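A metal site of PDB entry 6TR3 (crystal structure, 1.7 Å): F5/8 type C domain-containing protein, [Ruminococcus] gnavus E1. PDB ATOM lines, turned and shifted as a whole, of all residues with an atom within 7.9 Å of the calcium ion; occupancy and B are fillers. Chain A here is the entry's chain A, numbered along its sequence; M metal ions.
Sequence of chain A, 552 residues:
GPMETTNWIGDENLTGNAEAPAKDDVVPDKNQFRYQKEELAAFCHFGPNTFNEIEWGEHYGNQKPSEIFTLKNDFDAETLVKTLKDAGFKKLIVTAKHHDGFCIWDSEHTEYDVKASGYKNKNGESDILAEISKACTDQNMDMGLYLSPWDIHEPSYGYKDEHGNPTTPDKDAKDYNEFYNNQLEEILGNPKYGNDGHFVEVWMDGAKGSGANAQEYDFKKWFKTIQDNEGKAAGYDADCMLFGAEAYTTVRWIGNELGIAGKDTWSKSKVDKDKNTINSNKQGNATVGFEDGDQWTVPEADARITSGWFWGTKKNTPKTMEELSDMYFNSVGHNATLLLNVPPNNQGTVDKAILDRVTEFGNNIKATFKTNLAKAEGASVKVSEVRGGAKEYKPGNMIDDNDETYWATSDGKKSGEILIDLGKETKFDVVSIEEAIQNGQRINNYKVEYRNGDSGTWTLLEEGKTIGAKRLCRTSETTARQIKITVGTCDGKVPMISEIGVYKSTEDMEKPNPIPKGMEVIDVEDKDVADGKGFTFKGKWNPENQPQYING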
ATOM      1  N   LYS A 394     -11.392  -4.330 -25.738  1.00  0.00           N
ATOM      2  CA  LYS A 394     -11.827  -5.454 -26.578  1.00  0.00           C
ATOM      3  C   LYS A 394     -12.793  -4.996 -27.658  1.00  0.00           C
ATOM      4  O   LYS A 394     -13.523  -4.019 -27.477  1.00  0.00           O
ATOM      5  CB  LYS A 394     -12.503  -6.534 -25.715  1.00  0.00           C
ATOM      6  CG  LYS A 394     -13.848  -6.147 -25.115  1.00  0.00           C
ATOM      7  CD  LYS A 394     -14.361  -7.203 -24.151  1.00  0.00           C
ATOM      8  CE  LYS A 394     -15.841  -6.974 -23.870  1.00  0.00           C
ATOM      9  NZ  LYS A 394     -16.395  -7.908 -22.837  1.00  0.00           N
ATOM     10  N   PRO A 395     -12.848  -5.672 -28.833  1.00  0.00           N
ATOM     11  CA  PRO A 395     -13.741  -5.244 -29.911  1.00  0.00           C
ATOM     12  C   PRO A 395     -15.244  -5.233 -29.558  1.00  0.00           C
ATOM     13  O   PRO A 395     -16.007  -4.517 -30.213  1.00  0.00           O
ATOM     14  CB  PRO A 395     -13.442  -6.240 -31.040  1.00  0.00           C
ATOM     15  CG  PRO A 395     -12.709  -7.393 -30.396  1.00  0.00           C
ATOM     16  CD  PRO A 395     -12.034  -6.857 -29.175  1.00  0.00           C
ATOM     17  N   GLY A 396     -15.637  -6.028 -28.557  1.00  0.00           N
ATOM     18  CA  GLY A 396     -17.004  -6.073 -28.067  1.00  0.00           C
ATOM     19  C   GLY A 396     -17.470  -4.743 -27.479  1.00  0.00           C
ATOM     20  O   GLY A 396     -18.660  -4.525 -27.337  1.00  0.00           O
ATOM     21  N   ASN A 397     -16.513  -3.849 -27.178  1.00  0.00           N
ATOM     22  CA  ASN A 397     -16.803  -2.511 -26.708  1.00  0.00           C
ATOM     23  C   ASN A 397     -17.441  -1.636 -27.785  1.00  0.00           C
ATOM     24  O   ASN A 397     -17.994  -0.587 -27.473  1.00  0.00           O
ATOM     25  CB  ASN A 397     -15.541  -1.793 -26.202  1.00  0.00           C
ATOM     26  CG  ASN A 397     -15.020  -2.353 -24.850  1.00  0.00           C
ATOM     27  OD1 ASN A 397     -15.641  -3.190 -24.198  1.00  0.00           O
ATOM     28  ND2 ASN A 397     -13.894  -1.842 -24.418  1.00  0.00           N
ATOM     29  N   MET A 398     -17.354  -2.047 -29.056  1.00  0.00           N
ATOM     30  CA  MET A 398     -17.984  -1.287 -30.146  1.00  0.00           C
ATOM     31  C   MET A 398     -19.457  -1.639 -30.429  1.00  0.00           C
ATOM     32  O   MET A 398     -20.103  -1.021 -31.281  1.00  0.00           O
ATOM     33  CB  MET A 398     -17.172  -1.438 -31.428  1.00  0.00           C
ATOM     34  CG  MET A 398     -15.737  -0.945 -31.276  1.00  0.00           C
ATOM     35  SD  MET A 398     -14.818  -0.952 -32.813  1.00  0.00           S
ATOM     36  CE  MET A 398     -14.369  -2.691 -32.996  1.00  0.00           C
ATOM     37  N   ILE A 399     -19.982  -2.641 -29.712  1.00  0.00           N
ATOM     38  CA  ILE A 399     -21.361  -3.076 -29.860  1.00  0.00           C
ATOM     39  C   ILE A 399     -22.066  -3.311 -28.534  1.00  0.00           C
ATOM     40  O   ILE A 399     -22.966  -4.160 -28.451  1.00  0.00           O
ATOM     41  CB  ILE A 399     -21.446  -4.357 -30.752  1.00  0.00           C
ATOM     42  CG1 ILE A 399     -20.545  -5.458 -30.197  1.00  0.00           C
ATOM     43  CG2 ILE A 399     -21.077  -3.992 -32.184  1.00  0.00           C
ATOM     44  CD1 ILE A 399     -20.831  -6.832 -30.766  1.00  0.00           C
ATOM     45  N   ASP A 400     -21.680  -2.556 -27.505  1.00  0.00           N
ATOM     46  CA  ASP A 400     -22.295  -2.672 -26.180  1.00  0.00           C
ATOM     47  C   ASP A 400     -23.255  -1.532 -25.799  1.00  0.00           C
ATOM     48  O   ASP A 400     -23.702  -1.479 -24.667  1.00  0.00           O
ATOM     49  CB  ASP A 400     -21.219  -2.874 -25.099  1.00  0.00           C
ATOM     50  CG  ASP A 400     -20.290  -1.679 -24.943  1.00  0.00           C
ATOM     51  OD1 ASP A 400     -20.375  -0.709 -25.730  1.00  0.00           O
ATOM     52  OD2 ASP A 400     -19.440  -1.736 -24.020  1.00  0.00           O
ATOM     53  N   ASP A 401     -23.578  -0.653 -26.764  1.00  0.00           N
ATOM     54  CA  ASP A 401     -24.468   0.480 -26.540  1.00  0.00           C
ATOM     55  C   ASP A 401     -24.015   1.256 -25.300  1.00  0.00           C
ATOM     56  O   ASP A 401     -24.821   1.611 -24.457  1.00  0.00           O
ATOM     57  CB  ASP A 401     -25.931   0.033 -26.350  1.00  0.00           C
ATOM     58  CG  ASP A 401     -26.537  -0.551 -27.624  1.00  0.00           C
ATOM     59  OD1 ASP A 401     -26.326   0.014 -28.713  1.00  0.00           O
ATOM     60  OD2 ASP A 401     -27.253  -1.573 -27.504  1.00  0.00           O
ATOM     61  N   ASN A 402     -22.707   1.481 -25.207  1.00  0.00           N
ATOM     62  CA  ASN A 402     -22.108   2.218 -24.108  1.00  0.00           C
ATOM     63  C   ASN A 402     -21.074   3.168 -24.704  1.00  0.00           C
ATOM     64  O   ASN A 402     -20.040   2.759 -25.174  1.00  0.00           O
ATOM     65  CB  ASN A 402     -21.446   1.253 -23.110  1.00  0.00           C
ATOM     66  CG  ASN A 402     -21.019   1.941 -21.814  1.00  0.00           C
ATOM     67  OD1 ASN A 402     -20.850   3.144 -21.752  1.00  0.00           O
ATOM     68  ND2 ASN A 402     -20.831   1.148 -20.777  1.00  0.00           N
ATOM     69  N   ASP A 403     -21.370   4.464 -24.669  1.00  0.00           N
ATOM     70  CA  ASP A 403     -20.424   5.449 -25.180  1.00  0.00           C
ATOM     71  C   ASP A 403     -19.106   5.542 -24.427  1.00  0.00           C
ATOM     72  O   ASP A 403     -18.125   6.064 -24.973  1.00  0.00           O
ATOM     73  CB  ASP A 403     -21.090   6.824 -25.239  1.00  0.00           C
ATOM     74  CG  ASP A 403     -22.224   6.879 -26.230  1.00  0.00           C
ATOM     75  OD1 ASP A 403     -22.307   6.044 -27.146  1.00  0.00           O
ATOM     76  OD2 ASP A 403     -23.054   7.798 -26.062  1.00  0.00           O
ATOM     77  N   GLU A 404     -19.079   5.039 -23.184  1.00  0.00           N
ATOM     78  CA  GLU A 404     -17.894   5.108 -22.330  1.00  0.00           C
ATOM     79  C   GLU A 404     -16.830   4.044 -22.642  1.00  0.00           C
ATOM     80  O   GLU A 404     -15.674   4.198 -22.266  1.00  0.00           O
ATOM     81  CB  GLU A 404     -18.289   5.068 -20.849  1.00  0.00           C
ATOM     82  CG  GLU A 404     -19.200   6.234 -20.425  1.00  0.00           C
ATOM     83  CD  GLU A 404     -19.663   6.150 -18.971  1.00  0.00           C
ATOM     84  OE1 GLU A 404     -19.297   5.196 -18.253  1.00  0.00           O
ATOM     85  OE2 GLU A 404     -20.405   7.062 -18.522  1.00  0.00           O
ATOM     86  N   THR A 405     -17.239   2.955 -23.309  1.00  0.00           N
ATOM     87  CA  THR A 405     -16.326   1.864 -23.665  1.00  0.00           C
ATOM     88  C   THR A 405     -15.962   1.965 -25.131  1.00  0.00           C
ATOM     89  O   THR A 405     -16.828   2.265 -25.967  1.00  0.00           O
ATOM     90  CB  THR A 405     -16.983   0.480 -23.482  1.00  0.00           C
ATOM     91  OG1 THR A 405     -18.107   0.381 -24.352  1.00  0.00           O
ATOM     92  CG2 THR A 405     -17.413   0.233 -22.036  1.00  0.00           C
ATOM     93  N   TYR A 406     -14.694   1.688 -25.437  1.00  0.00           N
ATOM     94  CA  TYR A 406     -14.206   1.779 -26.806  1.00  0.00           C
ATOM     95  C   TYR A 406     -13.138   0.741 -27.083  1.00  0.00           C
ATOM     96  O   TYR A 406     -12.503   0.216 -26.170  1.00  0.00           O
ATOM     97  CB  TYR A 406     -13.662   3.189 -27.109  1.00  0.00           C
ATOM     98  CG  TYR A 406     -12.631   3.723 -26.133  1.00  0.00           C
ATOM     99  CD1 TYR A 406     -11.282   3.435 -26.284  1.00  0.00           C
ATOM    100  CD2 TYR A 406     -13.023   4.517 -25.051  1.00  0.00           C
ATOM    101  CE1 TYR A 406     -10.341   3.921 -25.390  1.00  0.00           C
ATOM    102  CE2 TYR A 406     -12.083   5.008 -24.141  1.00  0.00           C
ATOM    103  CZ  TYR A 406     -10.742   4.688 -24.319  1.00  0.00           C
ATOM    104  OH  TYR A 406      -9.799   5.155 -23.438  1.00  0.00           O
ATOM    105  N   TRP A 407     -12.967   0.441 -28.378  1.00  0.00           N
ATOM    106  CA  TRP A 407     -11.811  -0.279 -28.875  1.00  0.00           C
ATOM    107  C   TRP A 407     -10.720   0.734 -29.196  1.00  0.00           C
ATOM    108  O   TRP A 407     -11.005   1.853 -29.578  1.00  0.00           O
ATOM    109  CB  TRP A 407     -12.173  -1.099 -30.113  1.00  0.00           C
ATOM    110  CG  TRP A 407     -10.981  -1.508 -30.929  1.00  0.00           C
ATOM    111  CD1 TRP A 407     -10.065  -2.466 -30.611  1.00  0.00           C
ATOM    112  CD2 TRP A 407     -10.575  -0.974 -32.193  1.00  0.00           C
ATOM    113  NE1 TRP A 407      -9.112  -2.548 -31.595  1.00  0.00           N
ATOM    114  CE2 TRP A 407      -9.407  -1.653 -32.587  1.00  0.00           C
ATOM    115  CE3 TRP A 407     -11.086   0.015 -33.042  1.00  0.00           C
ATOM    116  CZ2 TRP A 407      -8.735  -1.379 -33.781  1.00  0.00           C
ATOM    117  CZ3 TRP A 407     -10.436   0.283 -34.224  1.00  0.00           C
ATOM    118  CH2 TRP A 407      -9.266  -0.417 -34.593  1.00  0.00           C
ATOM    119  N   GLU A 434     -18.673   5.481 -34.616  1.00  0.00           N
ATOM    120  CA  GLU A 434     -18.616   6.528 -33.586  1.00  0.00           C
ATOM    121  C   GLU A 434     -17.268   6.507 -32.875  1.00  0.00           C
ATOM    122  O   GLU A 434     -16.870   5.491 -32.292  1.00  0.00           O
ATOM    123  CB  GLU A 434     -19.762   6.362 -32.600  1.00  0.00           C
ATOM    124  CG  GLU A 434     -21.158   6.429 -33.250  1.00  0.00           C
ATOM    125  CD  GLU A 434     -22.282   6.092 -32.270  1.00  0.00           C
ATOM    126  OE1 GLU A 434     -22.337   6.722 -31.185  1.00  0.00           O
ATOM    127  OE2 GLU A 434     -23.107   5.203 -32.592  1.00  0.00           O
ATOM    128  N   GLN A 438     -15.147  11.981 -26.333  1.00  0.00           N
ATOM    129  CA  GLN A 438     -14.828  12.412 -24.971  1.00  0.00           C
ATOM    130  C   GLN A 438     -13.315  12.608 -24.794  1.00  0.00           C
ATOM    131  O   GLN A 438     -12.891  13.468 -24.031  1.00  0.00           O
ATOM    132  CB  GLN A 438     -15.388  11.476 -23.877  1.00  0.00           C
ATOM    133  CG  GLN A 438     -14.913  10.015 -23.872  1.00  0.00           C
ATOM    134  CD  GLN A 438     -15.837   9.103 -24.637  1.00  0.00           C
ATOM    135  OE1 GLN A 438     -16.247   9.407 -25.769  1.00  0.00           O
ATOM    136  NE2 GLN A 438     -16.189   7.978 -24.028  1.00  0.00           N
ATOM    137  N   ILE A 497     -12.717   3.877 -30.916  1.00  0.00           N
ATOM    138  CA  ILE A 497     -14.058   3.739 -31.498  1.00  0.00           C
ATOM    139  C   ILE A 497     -14.984   3.223 -30.411  1.00  0.00           C
ATOM    140  O   ILE A 497     -14.791   2.111 -29.911  1.00  0.00           O
ATOM    141  CB  ILE A 497     -14.027   2.733 -32.680  1.00  0.00           C
ATOM    142  CG1 ILE A 497     -13.072   3.244 -33.769  1.00  0.00           C
ATOM    143  CG2 ILE A 497     -15.414   2.512 -33.252  1.00  0.00           C
ATOM    144  CD1 ILE A 497     -13.416   4.609 -34.299  1.00  0.00           C
ATOM    145  N   SER A 498     -15.969   4.034 -30.026  1.00  0.00           N
ATOM    146  CA  SER A 498     -16.912   3.622 -28.979  1.00  0.00           C
ATOM    147  C   SER A 498     -18.096   2.770 -29.461  1.00  0.00           C
ATOM    148  O   SER A 498     -18.616   1.987 -28.691  1.00  0.00           O
ATOM    149  CB  SER A 498     -17.407   4.824 -28.177  1.00  0.00           C
ATOM    150  OG  SER A 498     -17.776   5.910 -29.016  1.00  0.00           O
ATOM    151  N   GLU A 499     -18.542   2.951 -30.714  1.00  0.00           N
ATOM    152  CA  GLU A 499     -19.641   2.139 -31.256  1.00  0.00           C
ATOM    153  C   GLU A 499     -19.551   2.038 -32.770  1.00  0.00           C
ATOM    154  O   GLU A 499     -19.108   2.989 -33.459  1.00  0.00           O
ATOM    155  CB  GLU A 499     -21.046   2.701 -30.910  1.00  0.00           C
ATOM    156  CG  GLU A 499     -21.430   2.794 -29.433  1.00  0.00           C
ATOM    157  CD  GLU A 499     -21.607   1.445 -28.735  1.00  0.00           C
ATOM    158  OE1 GLU A 499     -22.281   0.528 -29.280  1.00  0.00           O
ATOM    159  OE2 GLU A 499     -21.099   1.314 -27.602  1.00  0.00           O
ATOM    160  N   ILE A 500     -19.975   0.886 -33.303  1.00  0.00           N
ATOM    161  CA  ILE A 500     -20.183   0.684 -34.722  1.00  0.00           C
ATOM    162  C   ILE A 500     -21.481  -0.093 -34.915  1.00  0.00           C
ATOM    163  O   ILE A 500     -21.946  -0.793 -34.015  1.00  0.00           O
ATOM    164  CB  ILE A 500     -19.039  -0.127 -35.386  1.00  0.00           C
ATOM    165  CG1 ILE A 500     -18.982  -1.546 -34.830  1.00  0.00           C
ATOM    166  CG2 ILE A 500     -17.709   0.583 -35.225  1.00  0.00           C
ATOM    167  CD1 ILE A 500     -17.950  -2.432 -35.485  1.00  0.00           C
HETATM  168 CA    CA M   1     -18.966   1.095 -26.438  1.00  0.00          CA
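O of Tyr 406 sits at hydrogen-bond distance from ND2 of Asn 397 (3.0 Å). The side-chain amide oxygen (OD1) of Asn 402 lies within hydrogen-bond range of the backbone NH (N) of Glu 404 (3.0 Å). N of Asp 401 lies within hydrogen-bond range of OE1 of Glu 499 (3.1 Å). O of Glu 499 sits at hydrogen-bond distance from N of Glu 434 (2.8 Å). The backbone NH of Ser 498 is in hydrogen-bond range of the backbone carbonyl oxygen of Glu 434 (2.8 Å).
Of the 20 residues printed, 6 come within 4 Å of the calcium ion.
The calcium ion is bound by the backbone carbonyl oxygen (O) of Asn 397 (2.2 Å), the backbone carbonyl oxygen (O) of Asn 402 (2.3 Å), the side-chain hydroxyl (OG1) of Thr 405 (2.4 Å), the side-chain carboxylate (OD1) of Asp 400 (2.4 Å), the side-chain carboxylate (OE2) of Glu 499 (2.4 Å), the backbone carbonyl oxygen (O) of Ser 498 (2.4 Å) and the backbone carbonyl oxygen (O) of Thr 405 (2.5 Å). The calcium ion has seven donor atoms within binding distance.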
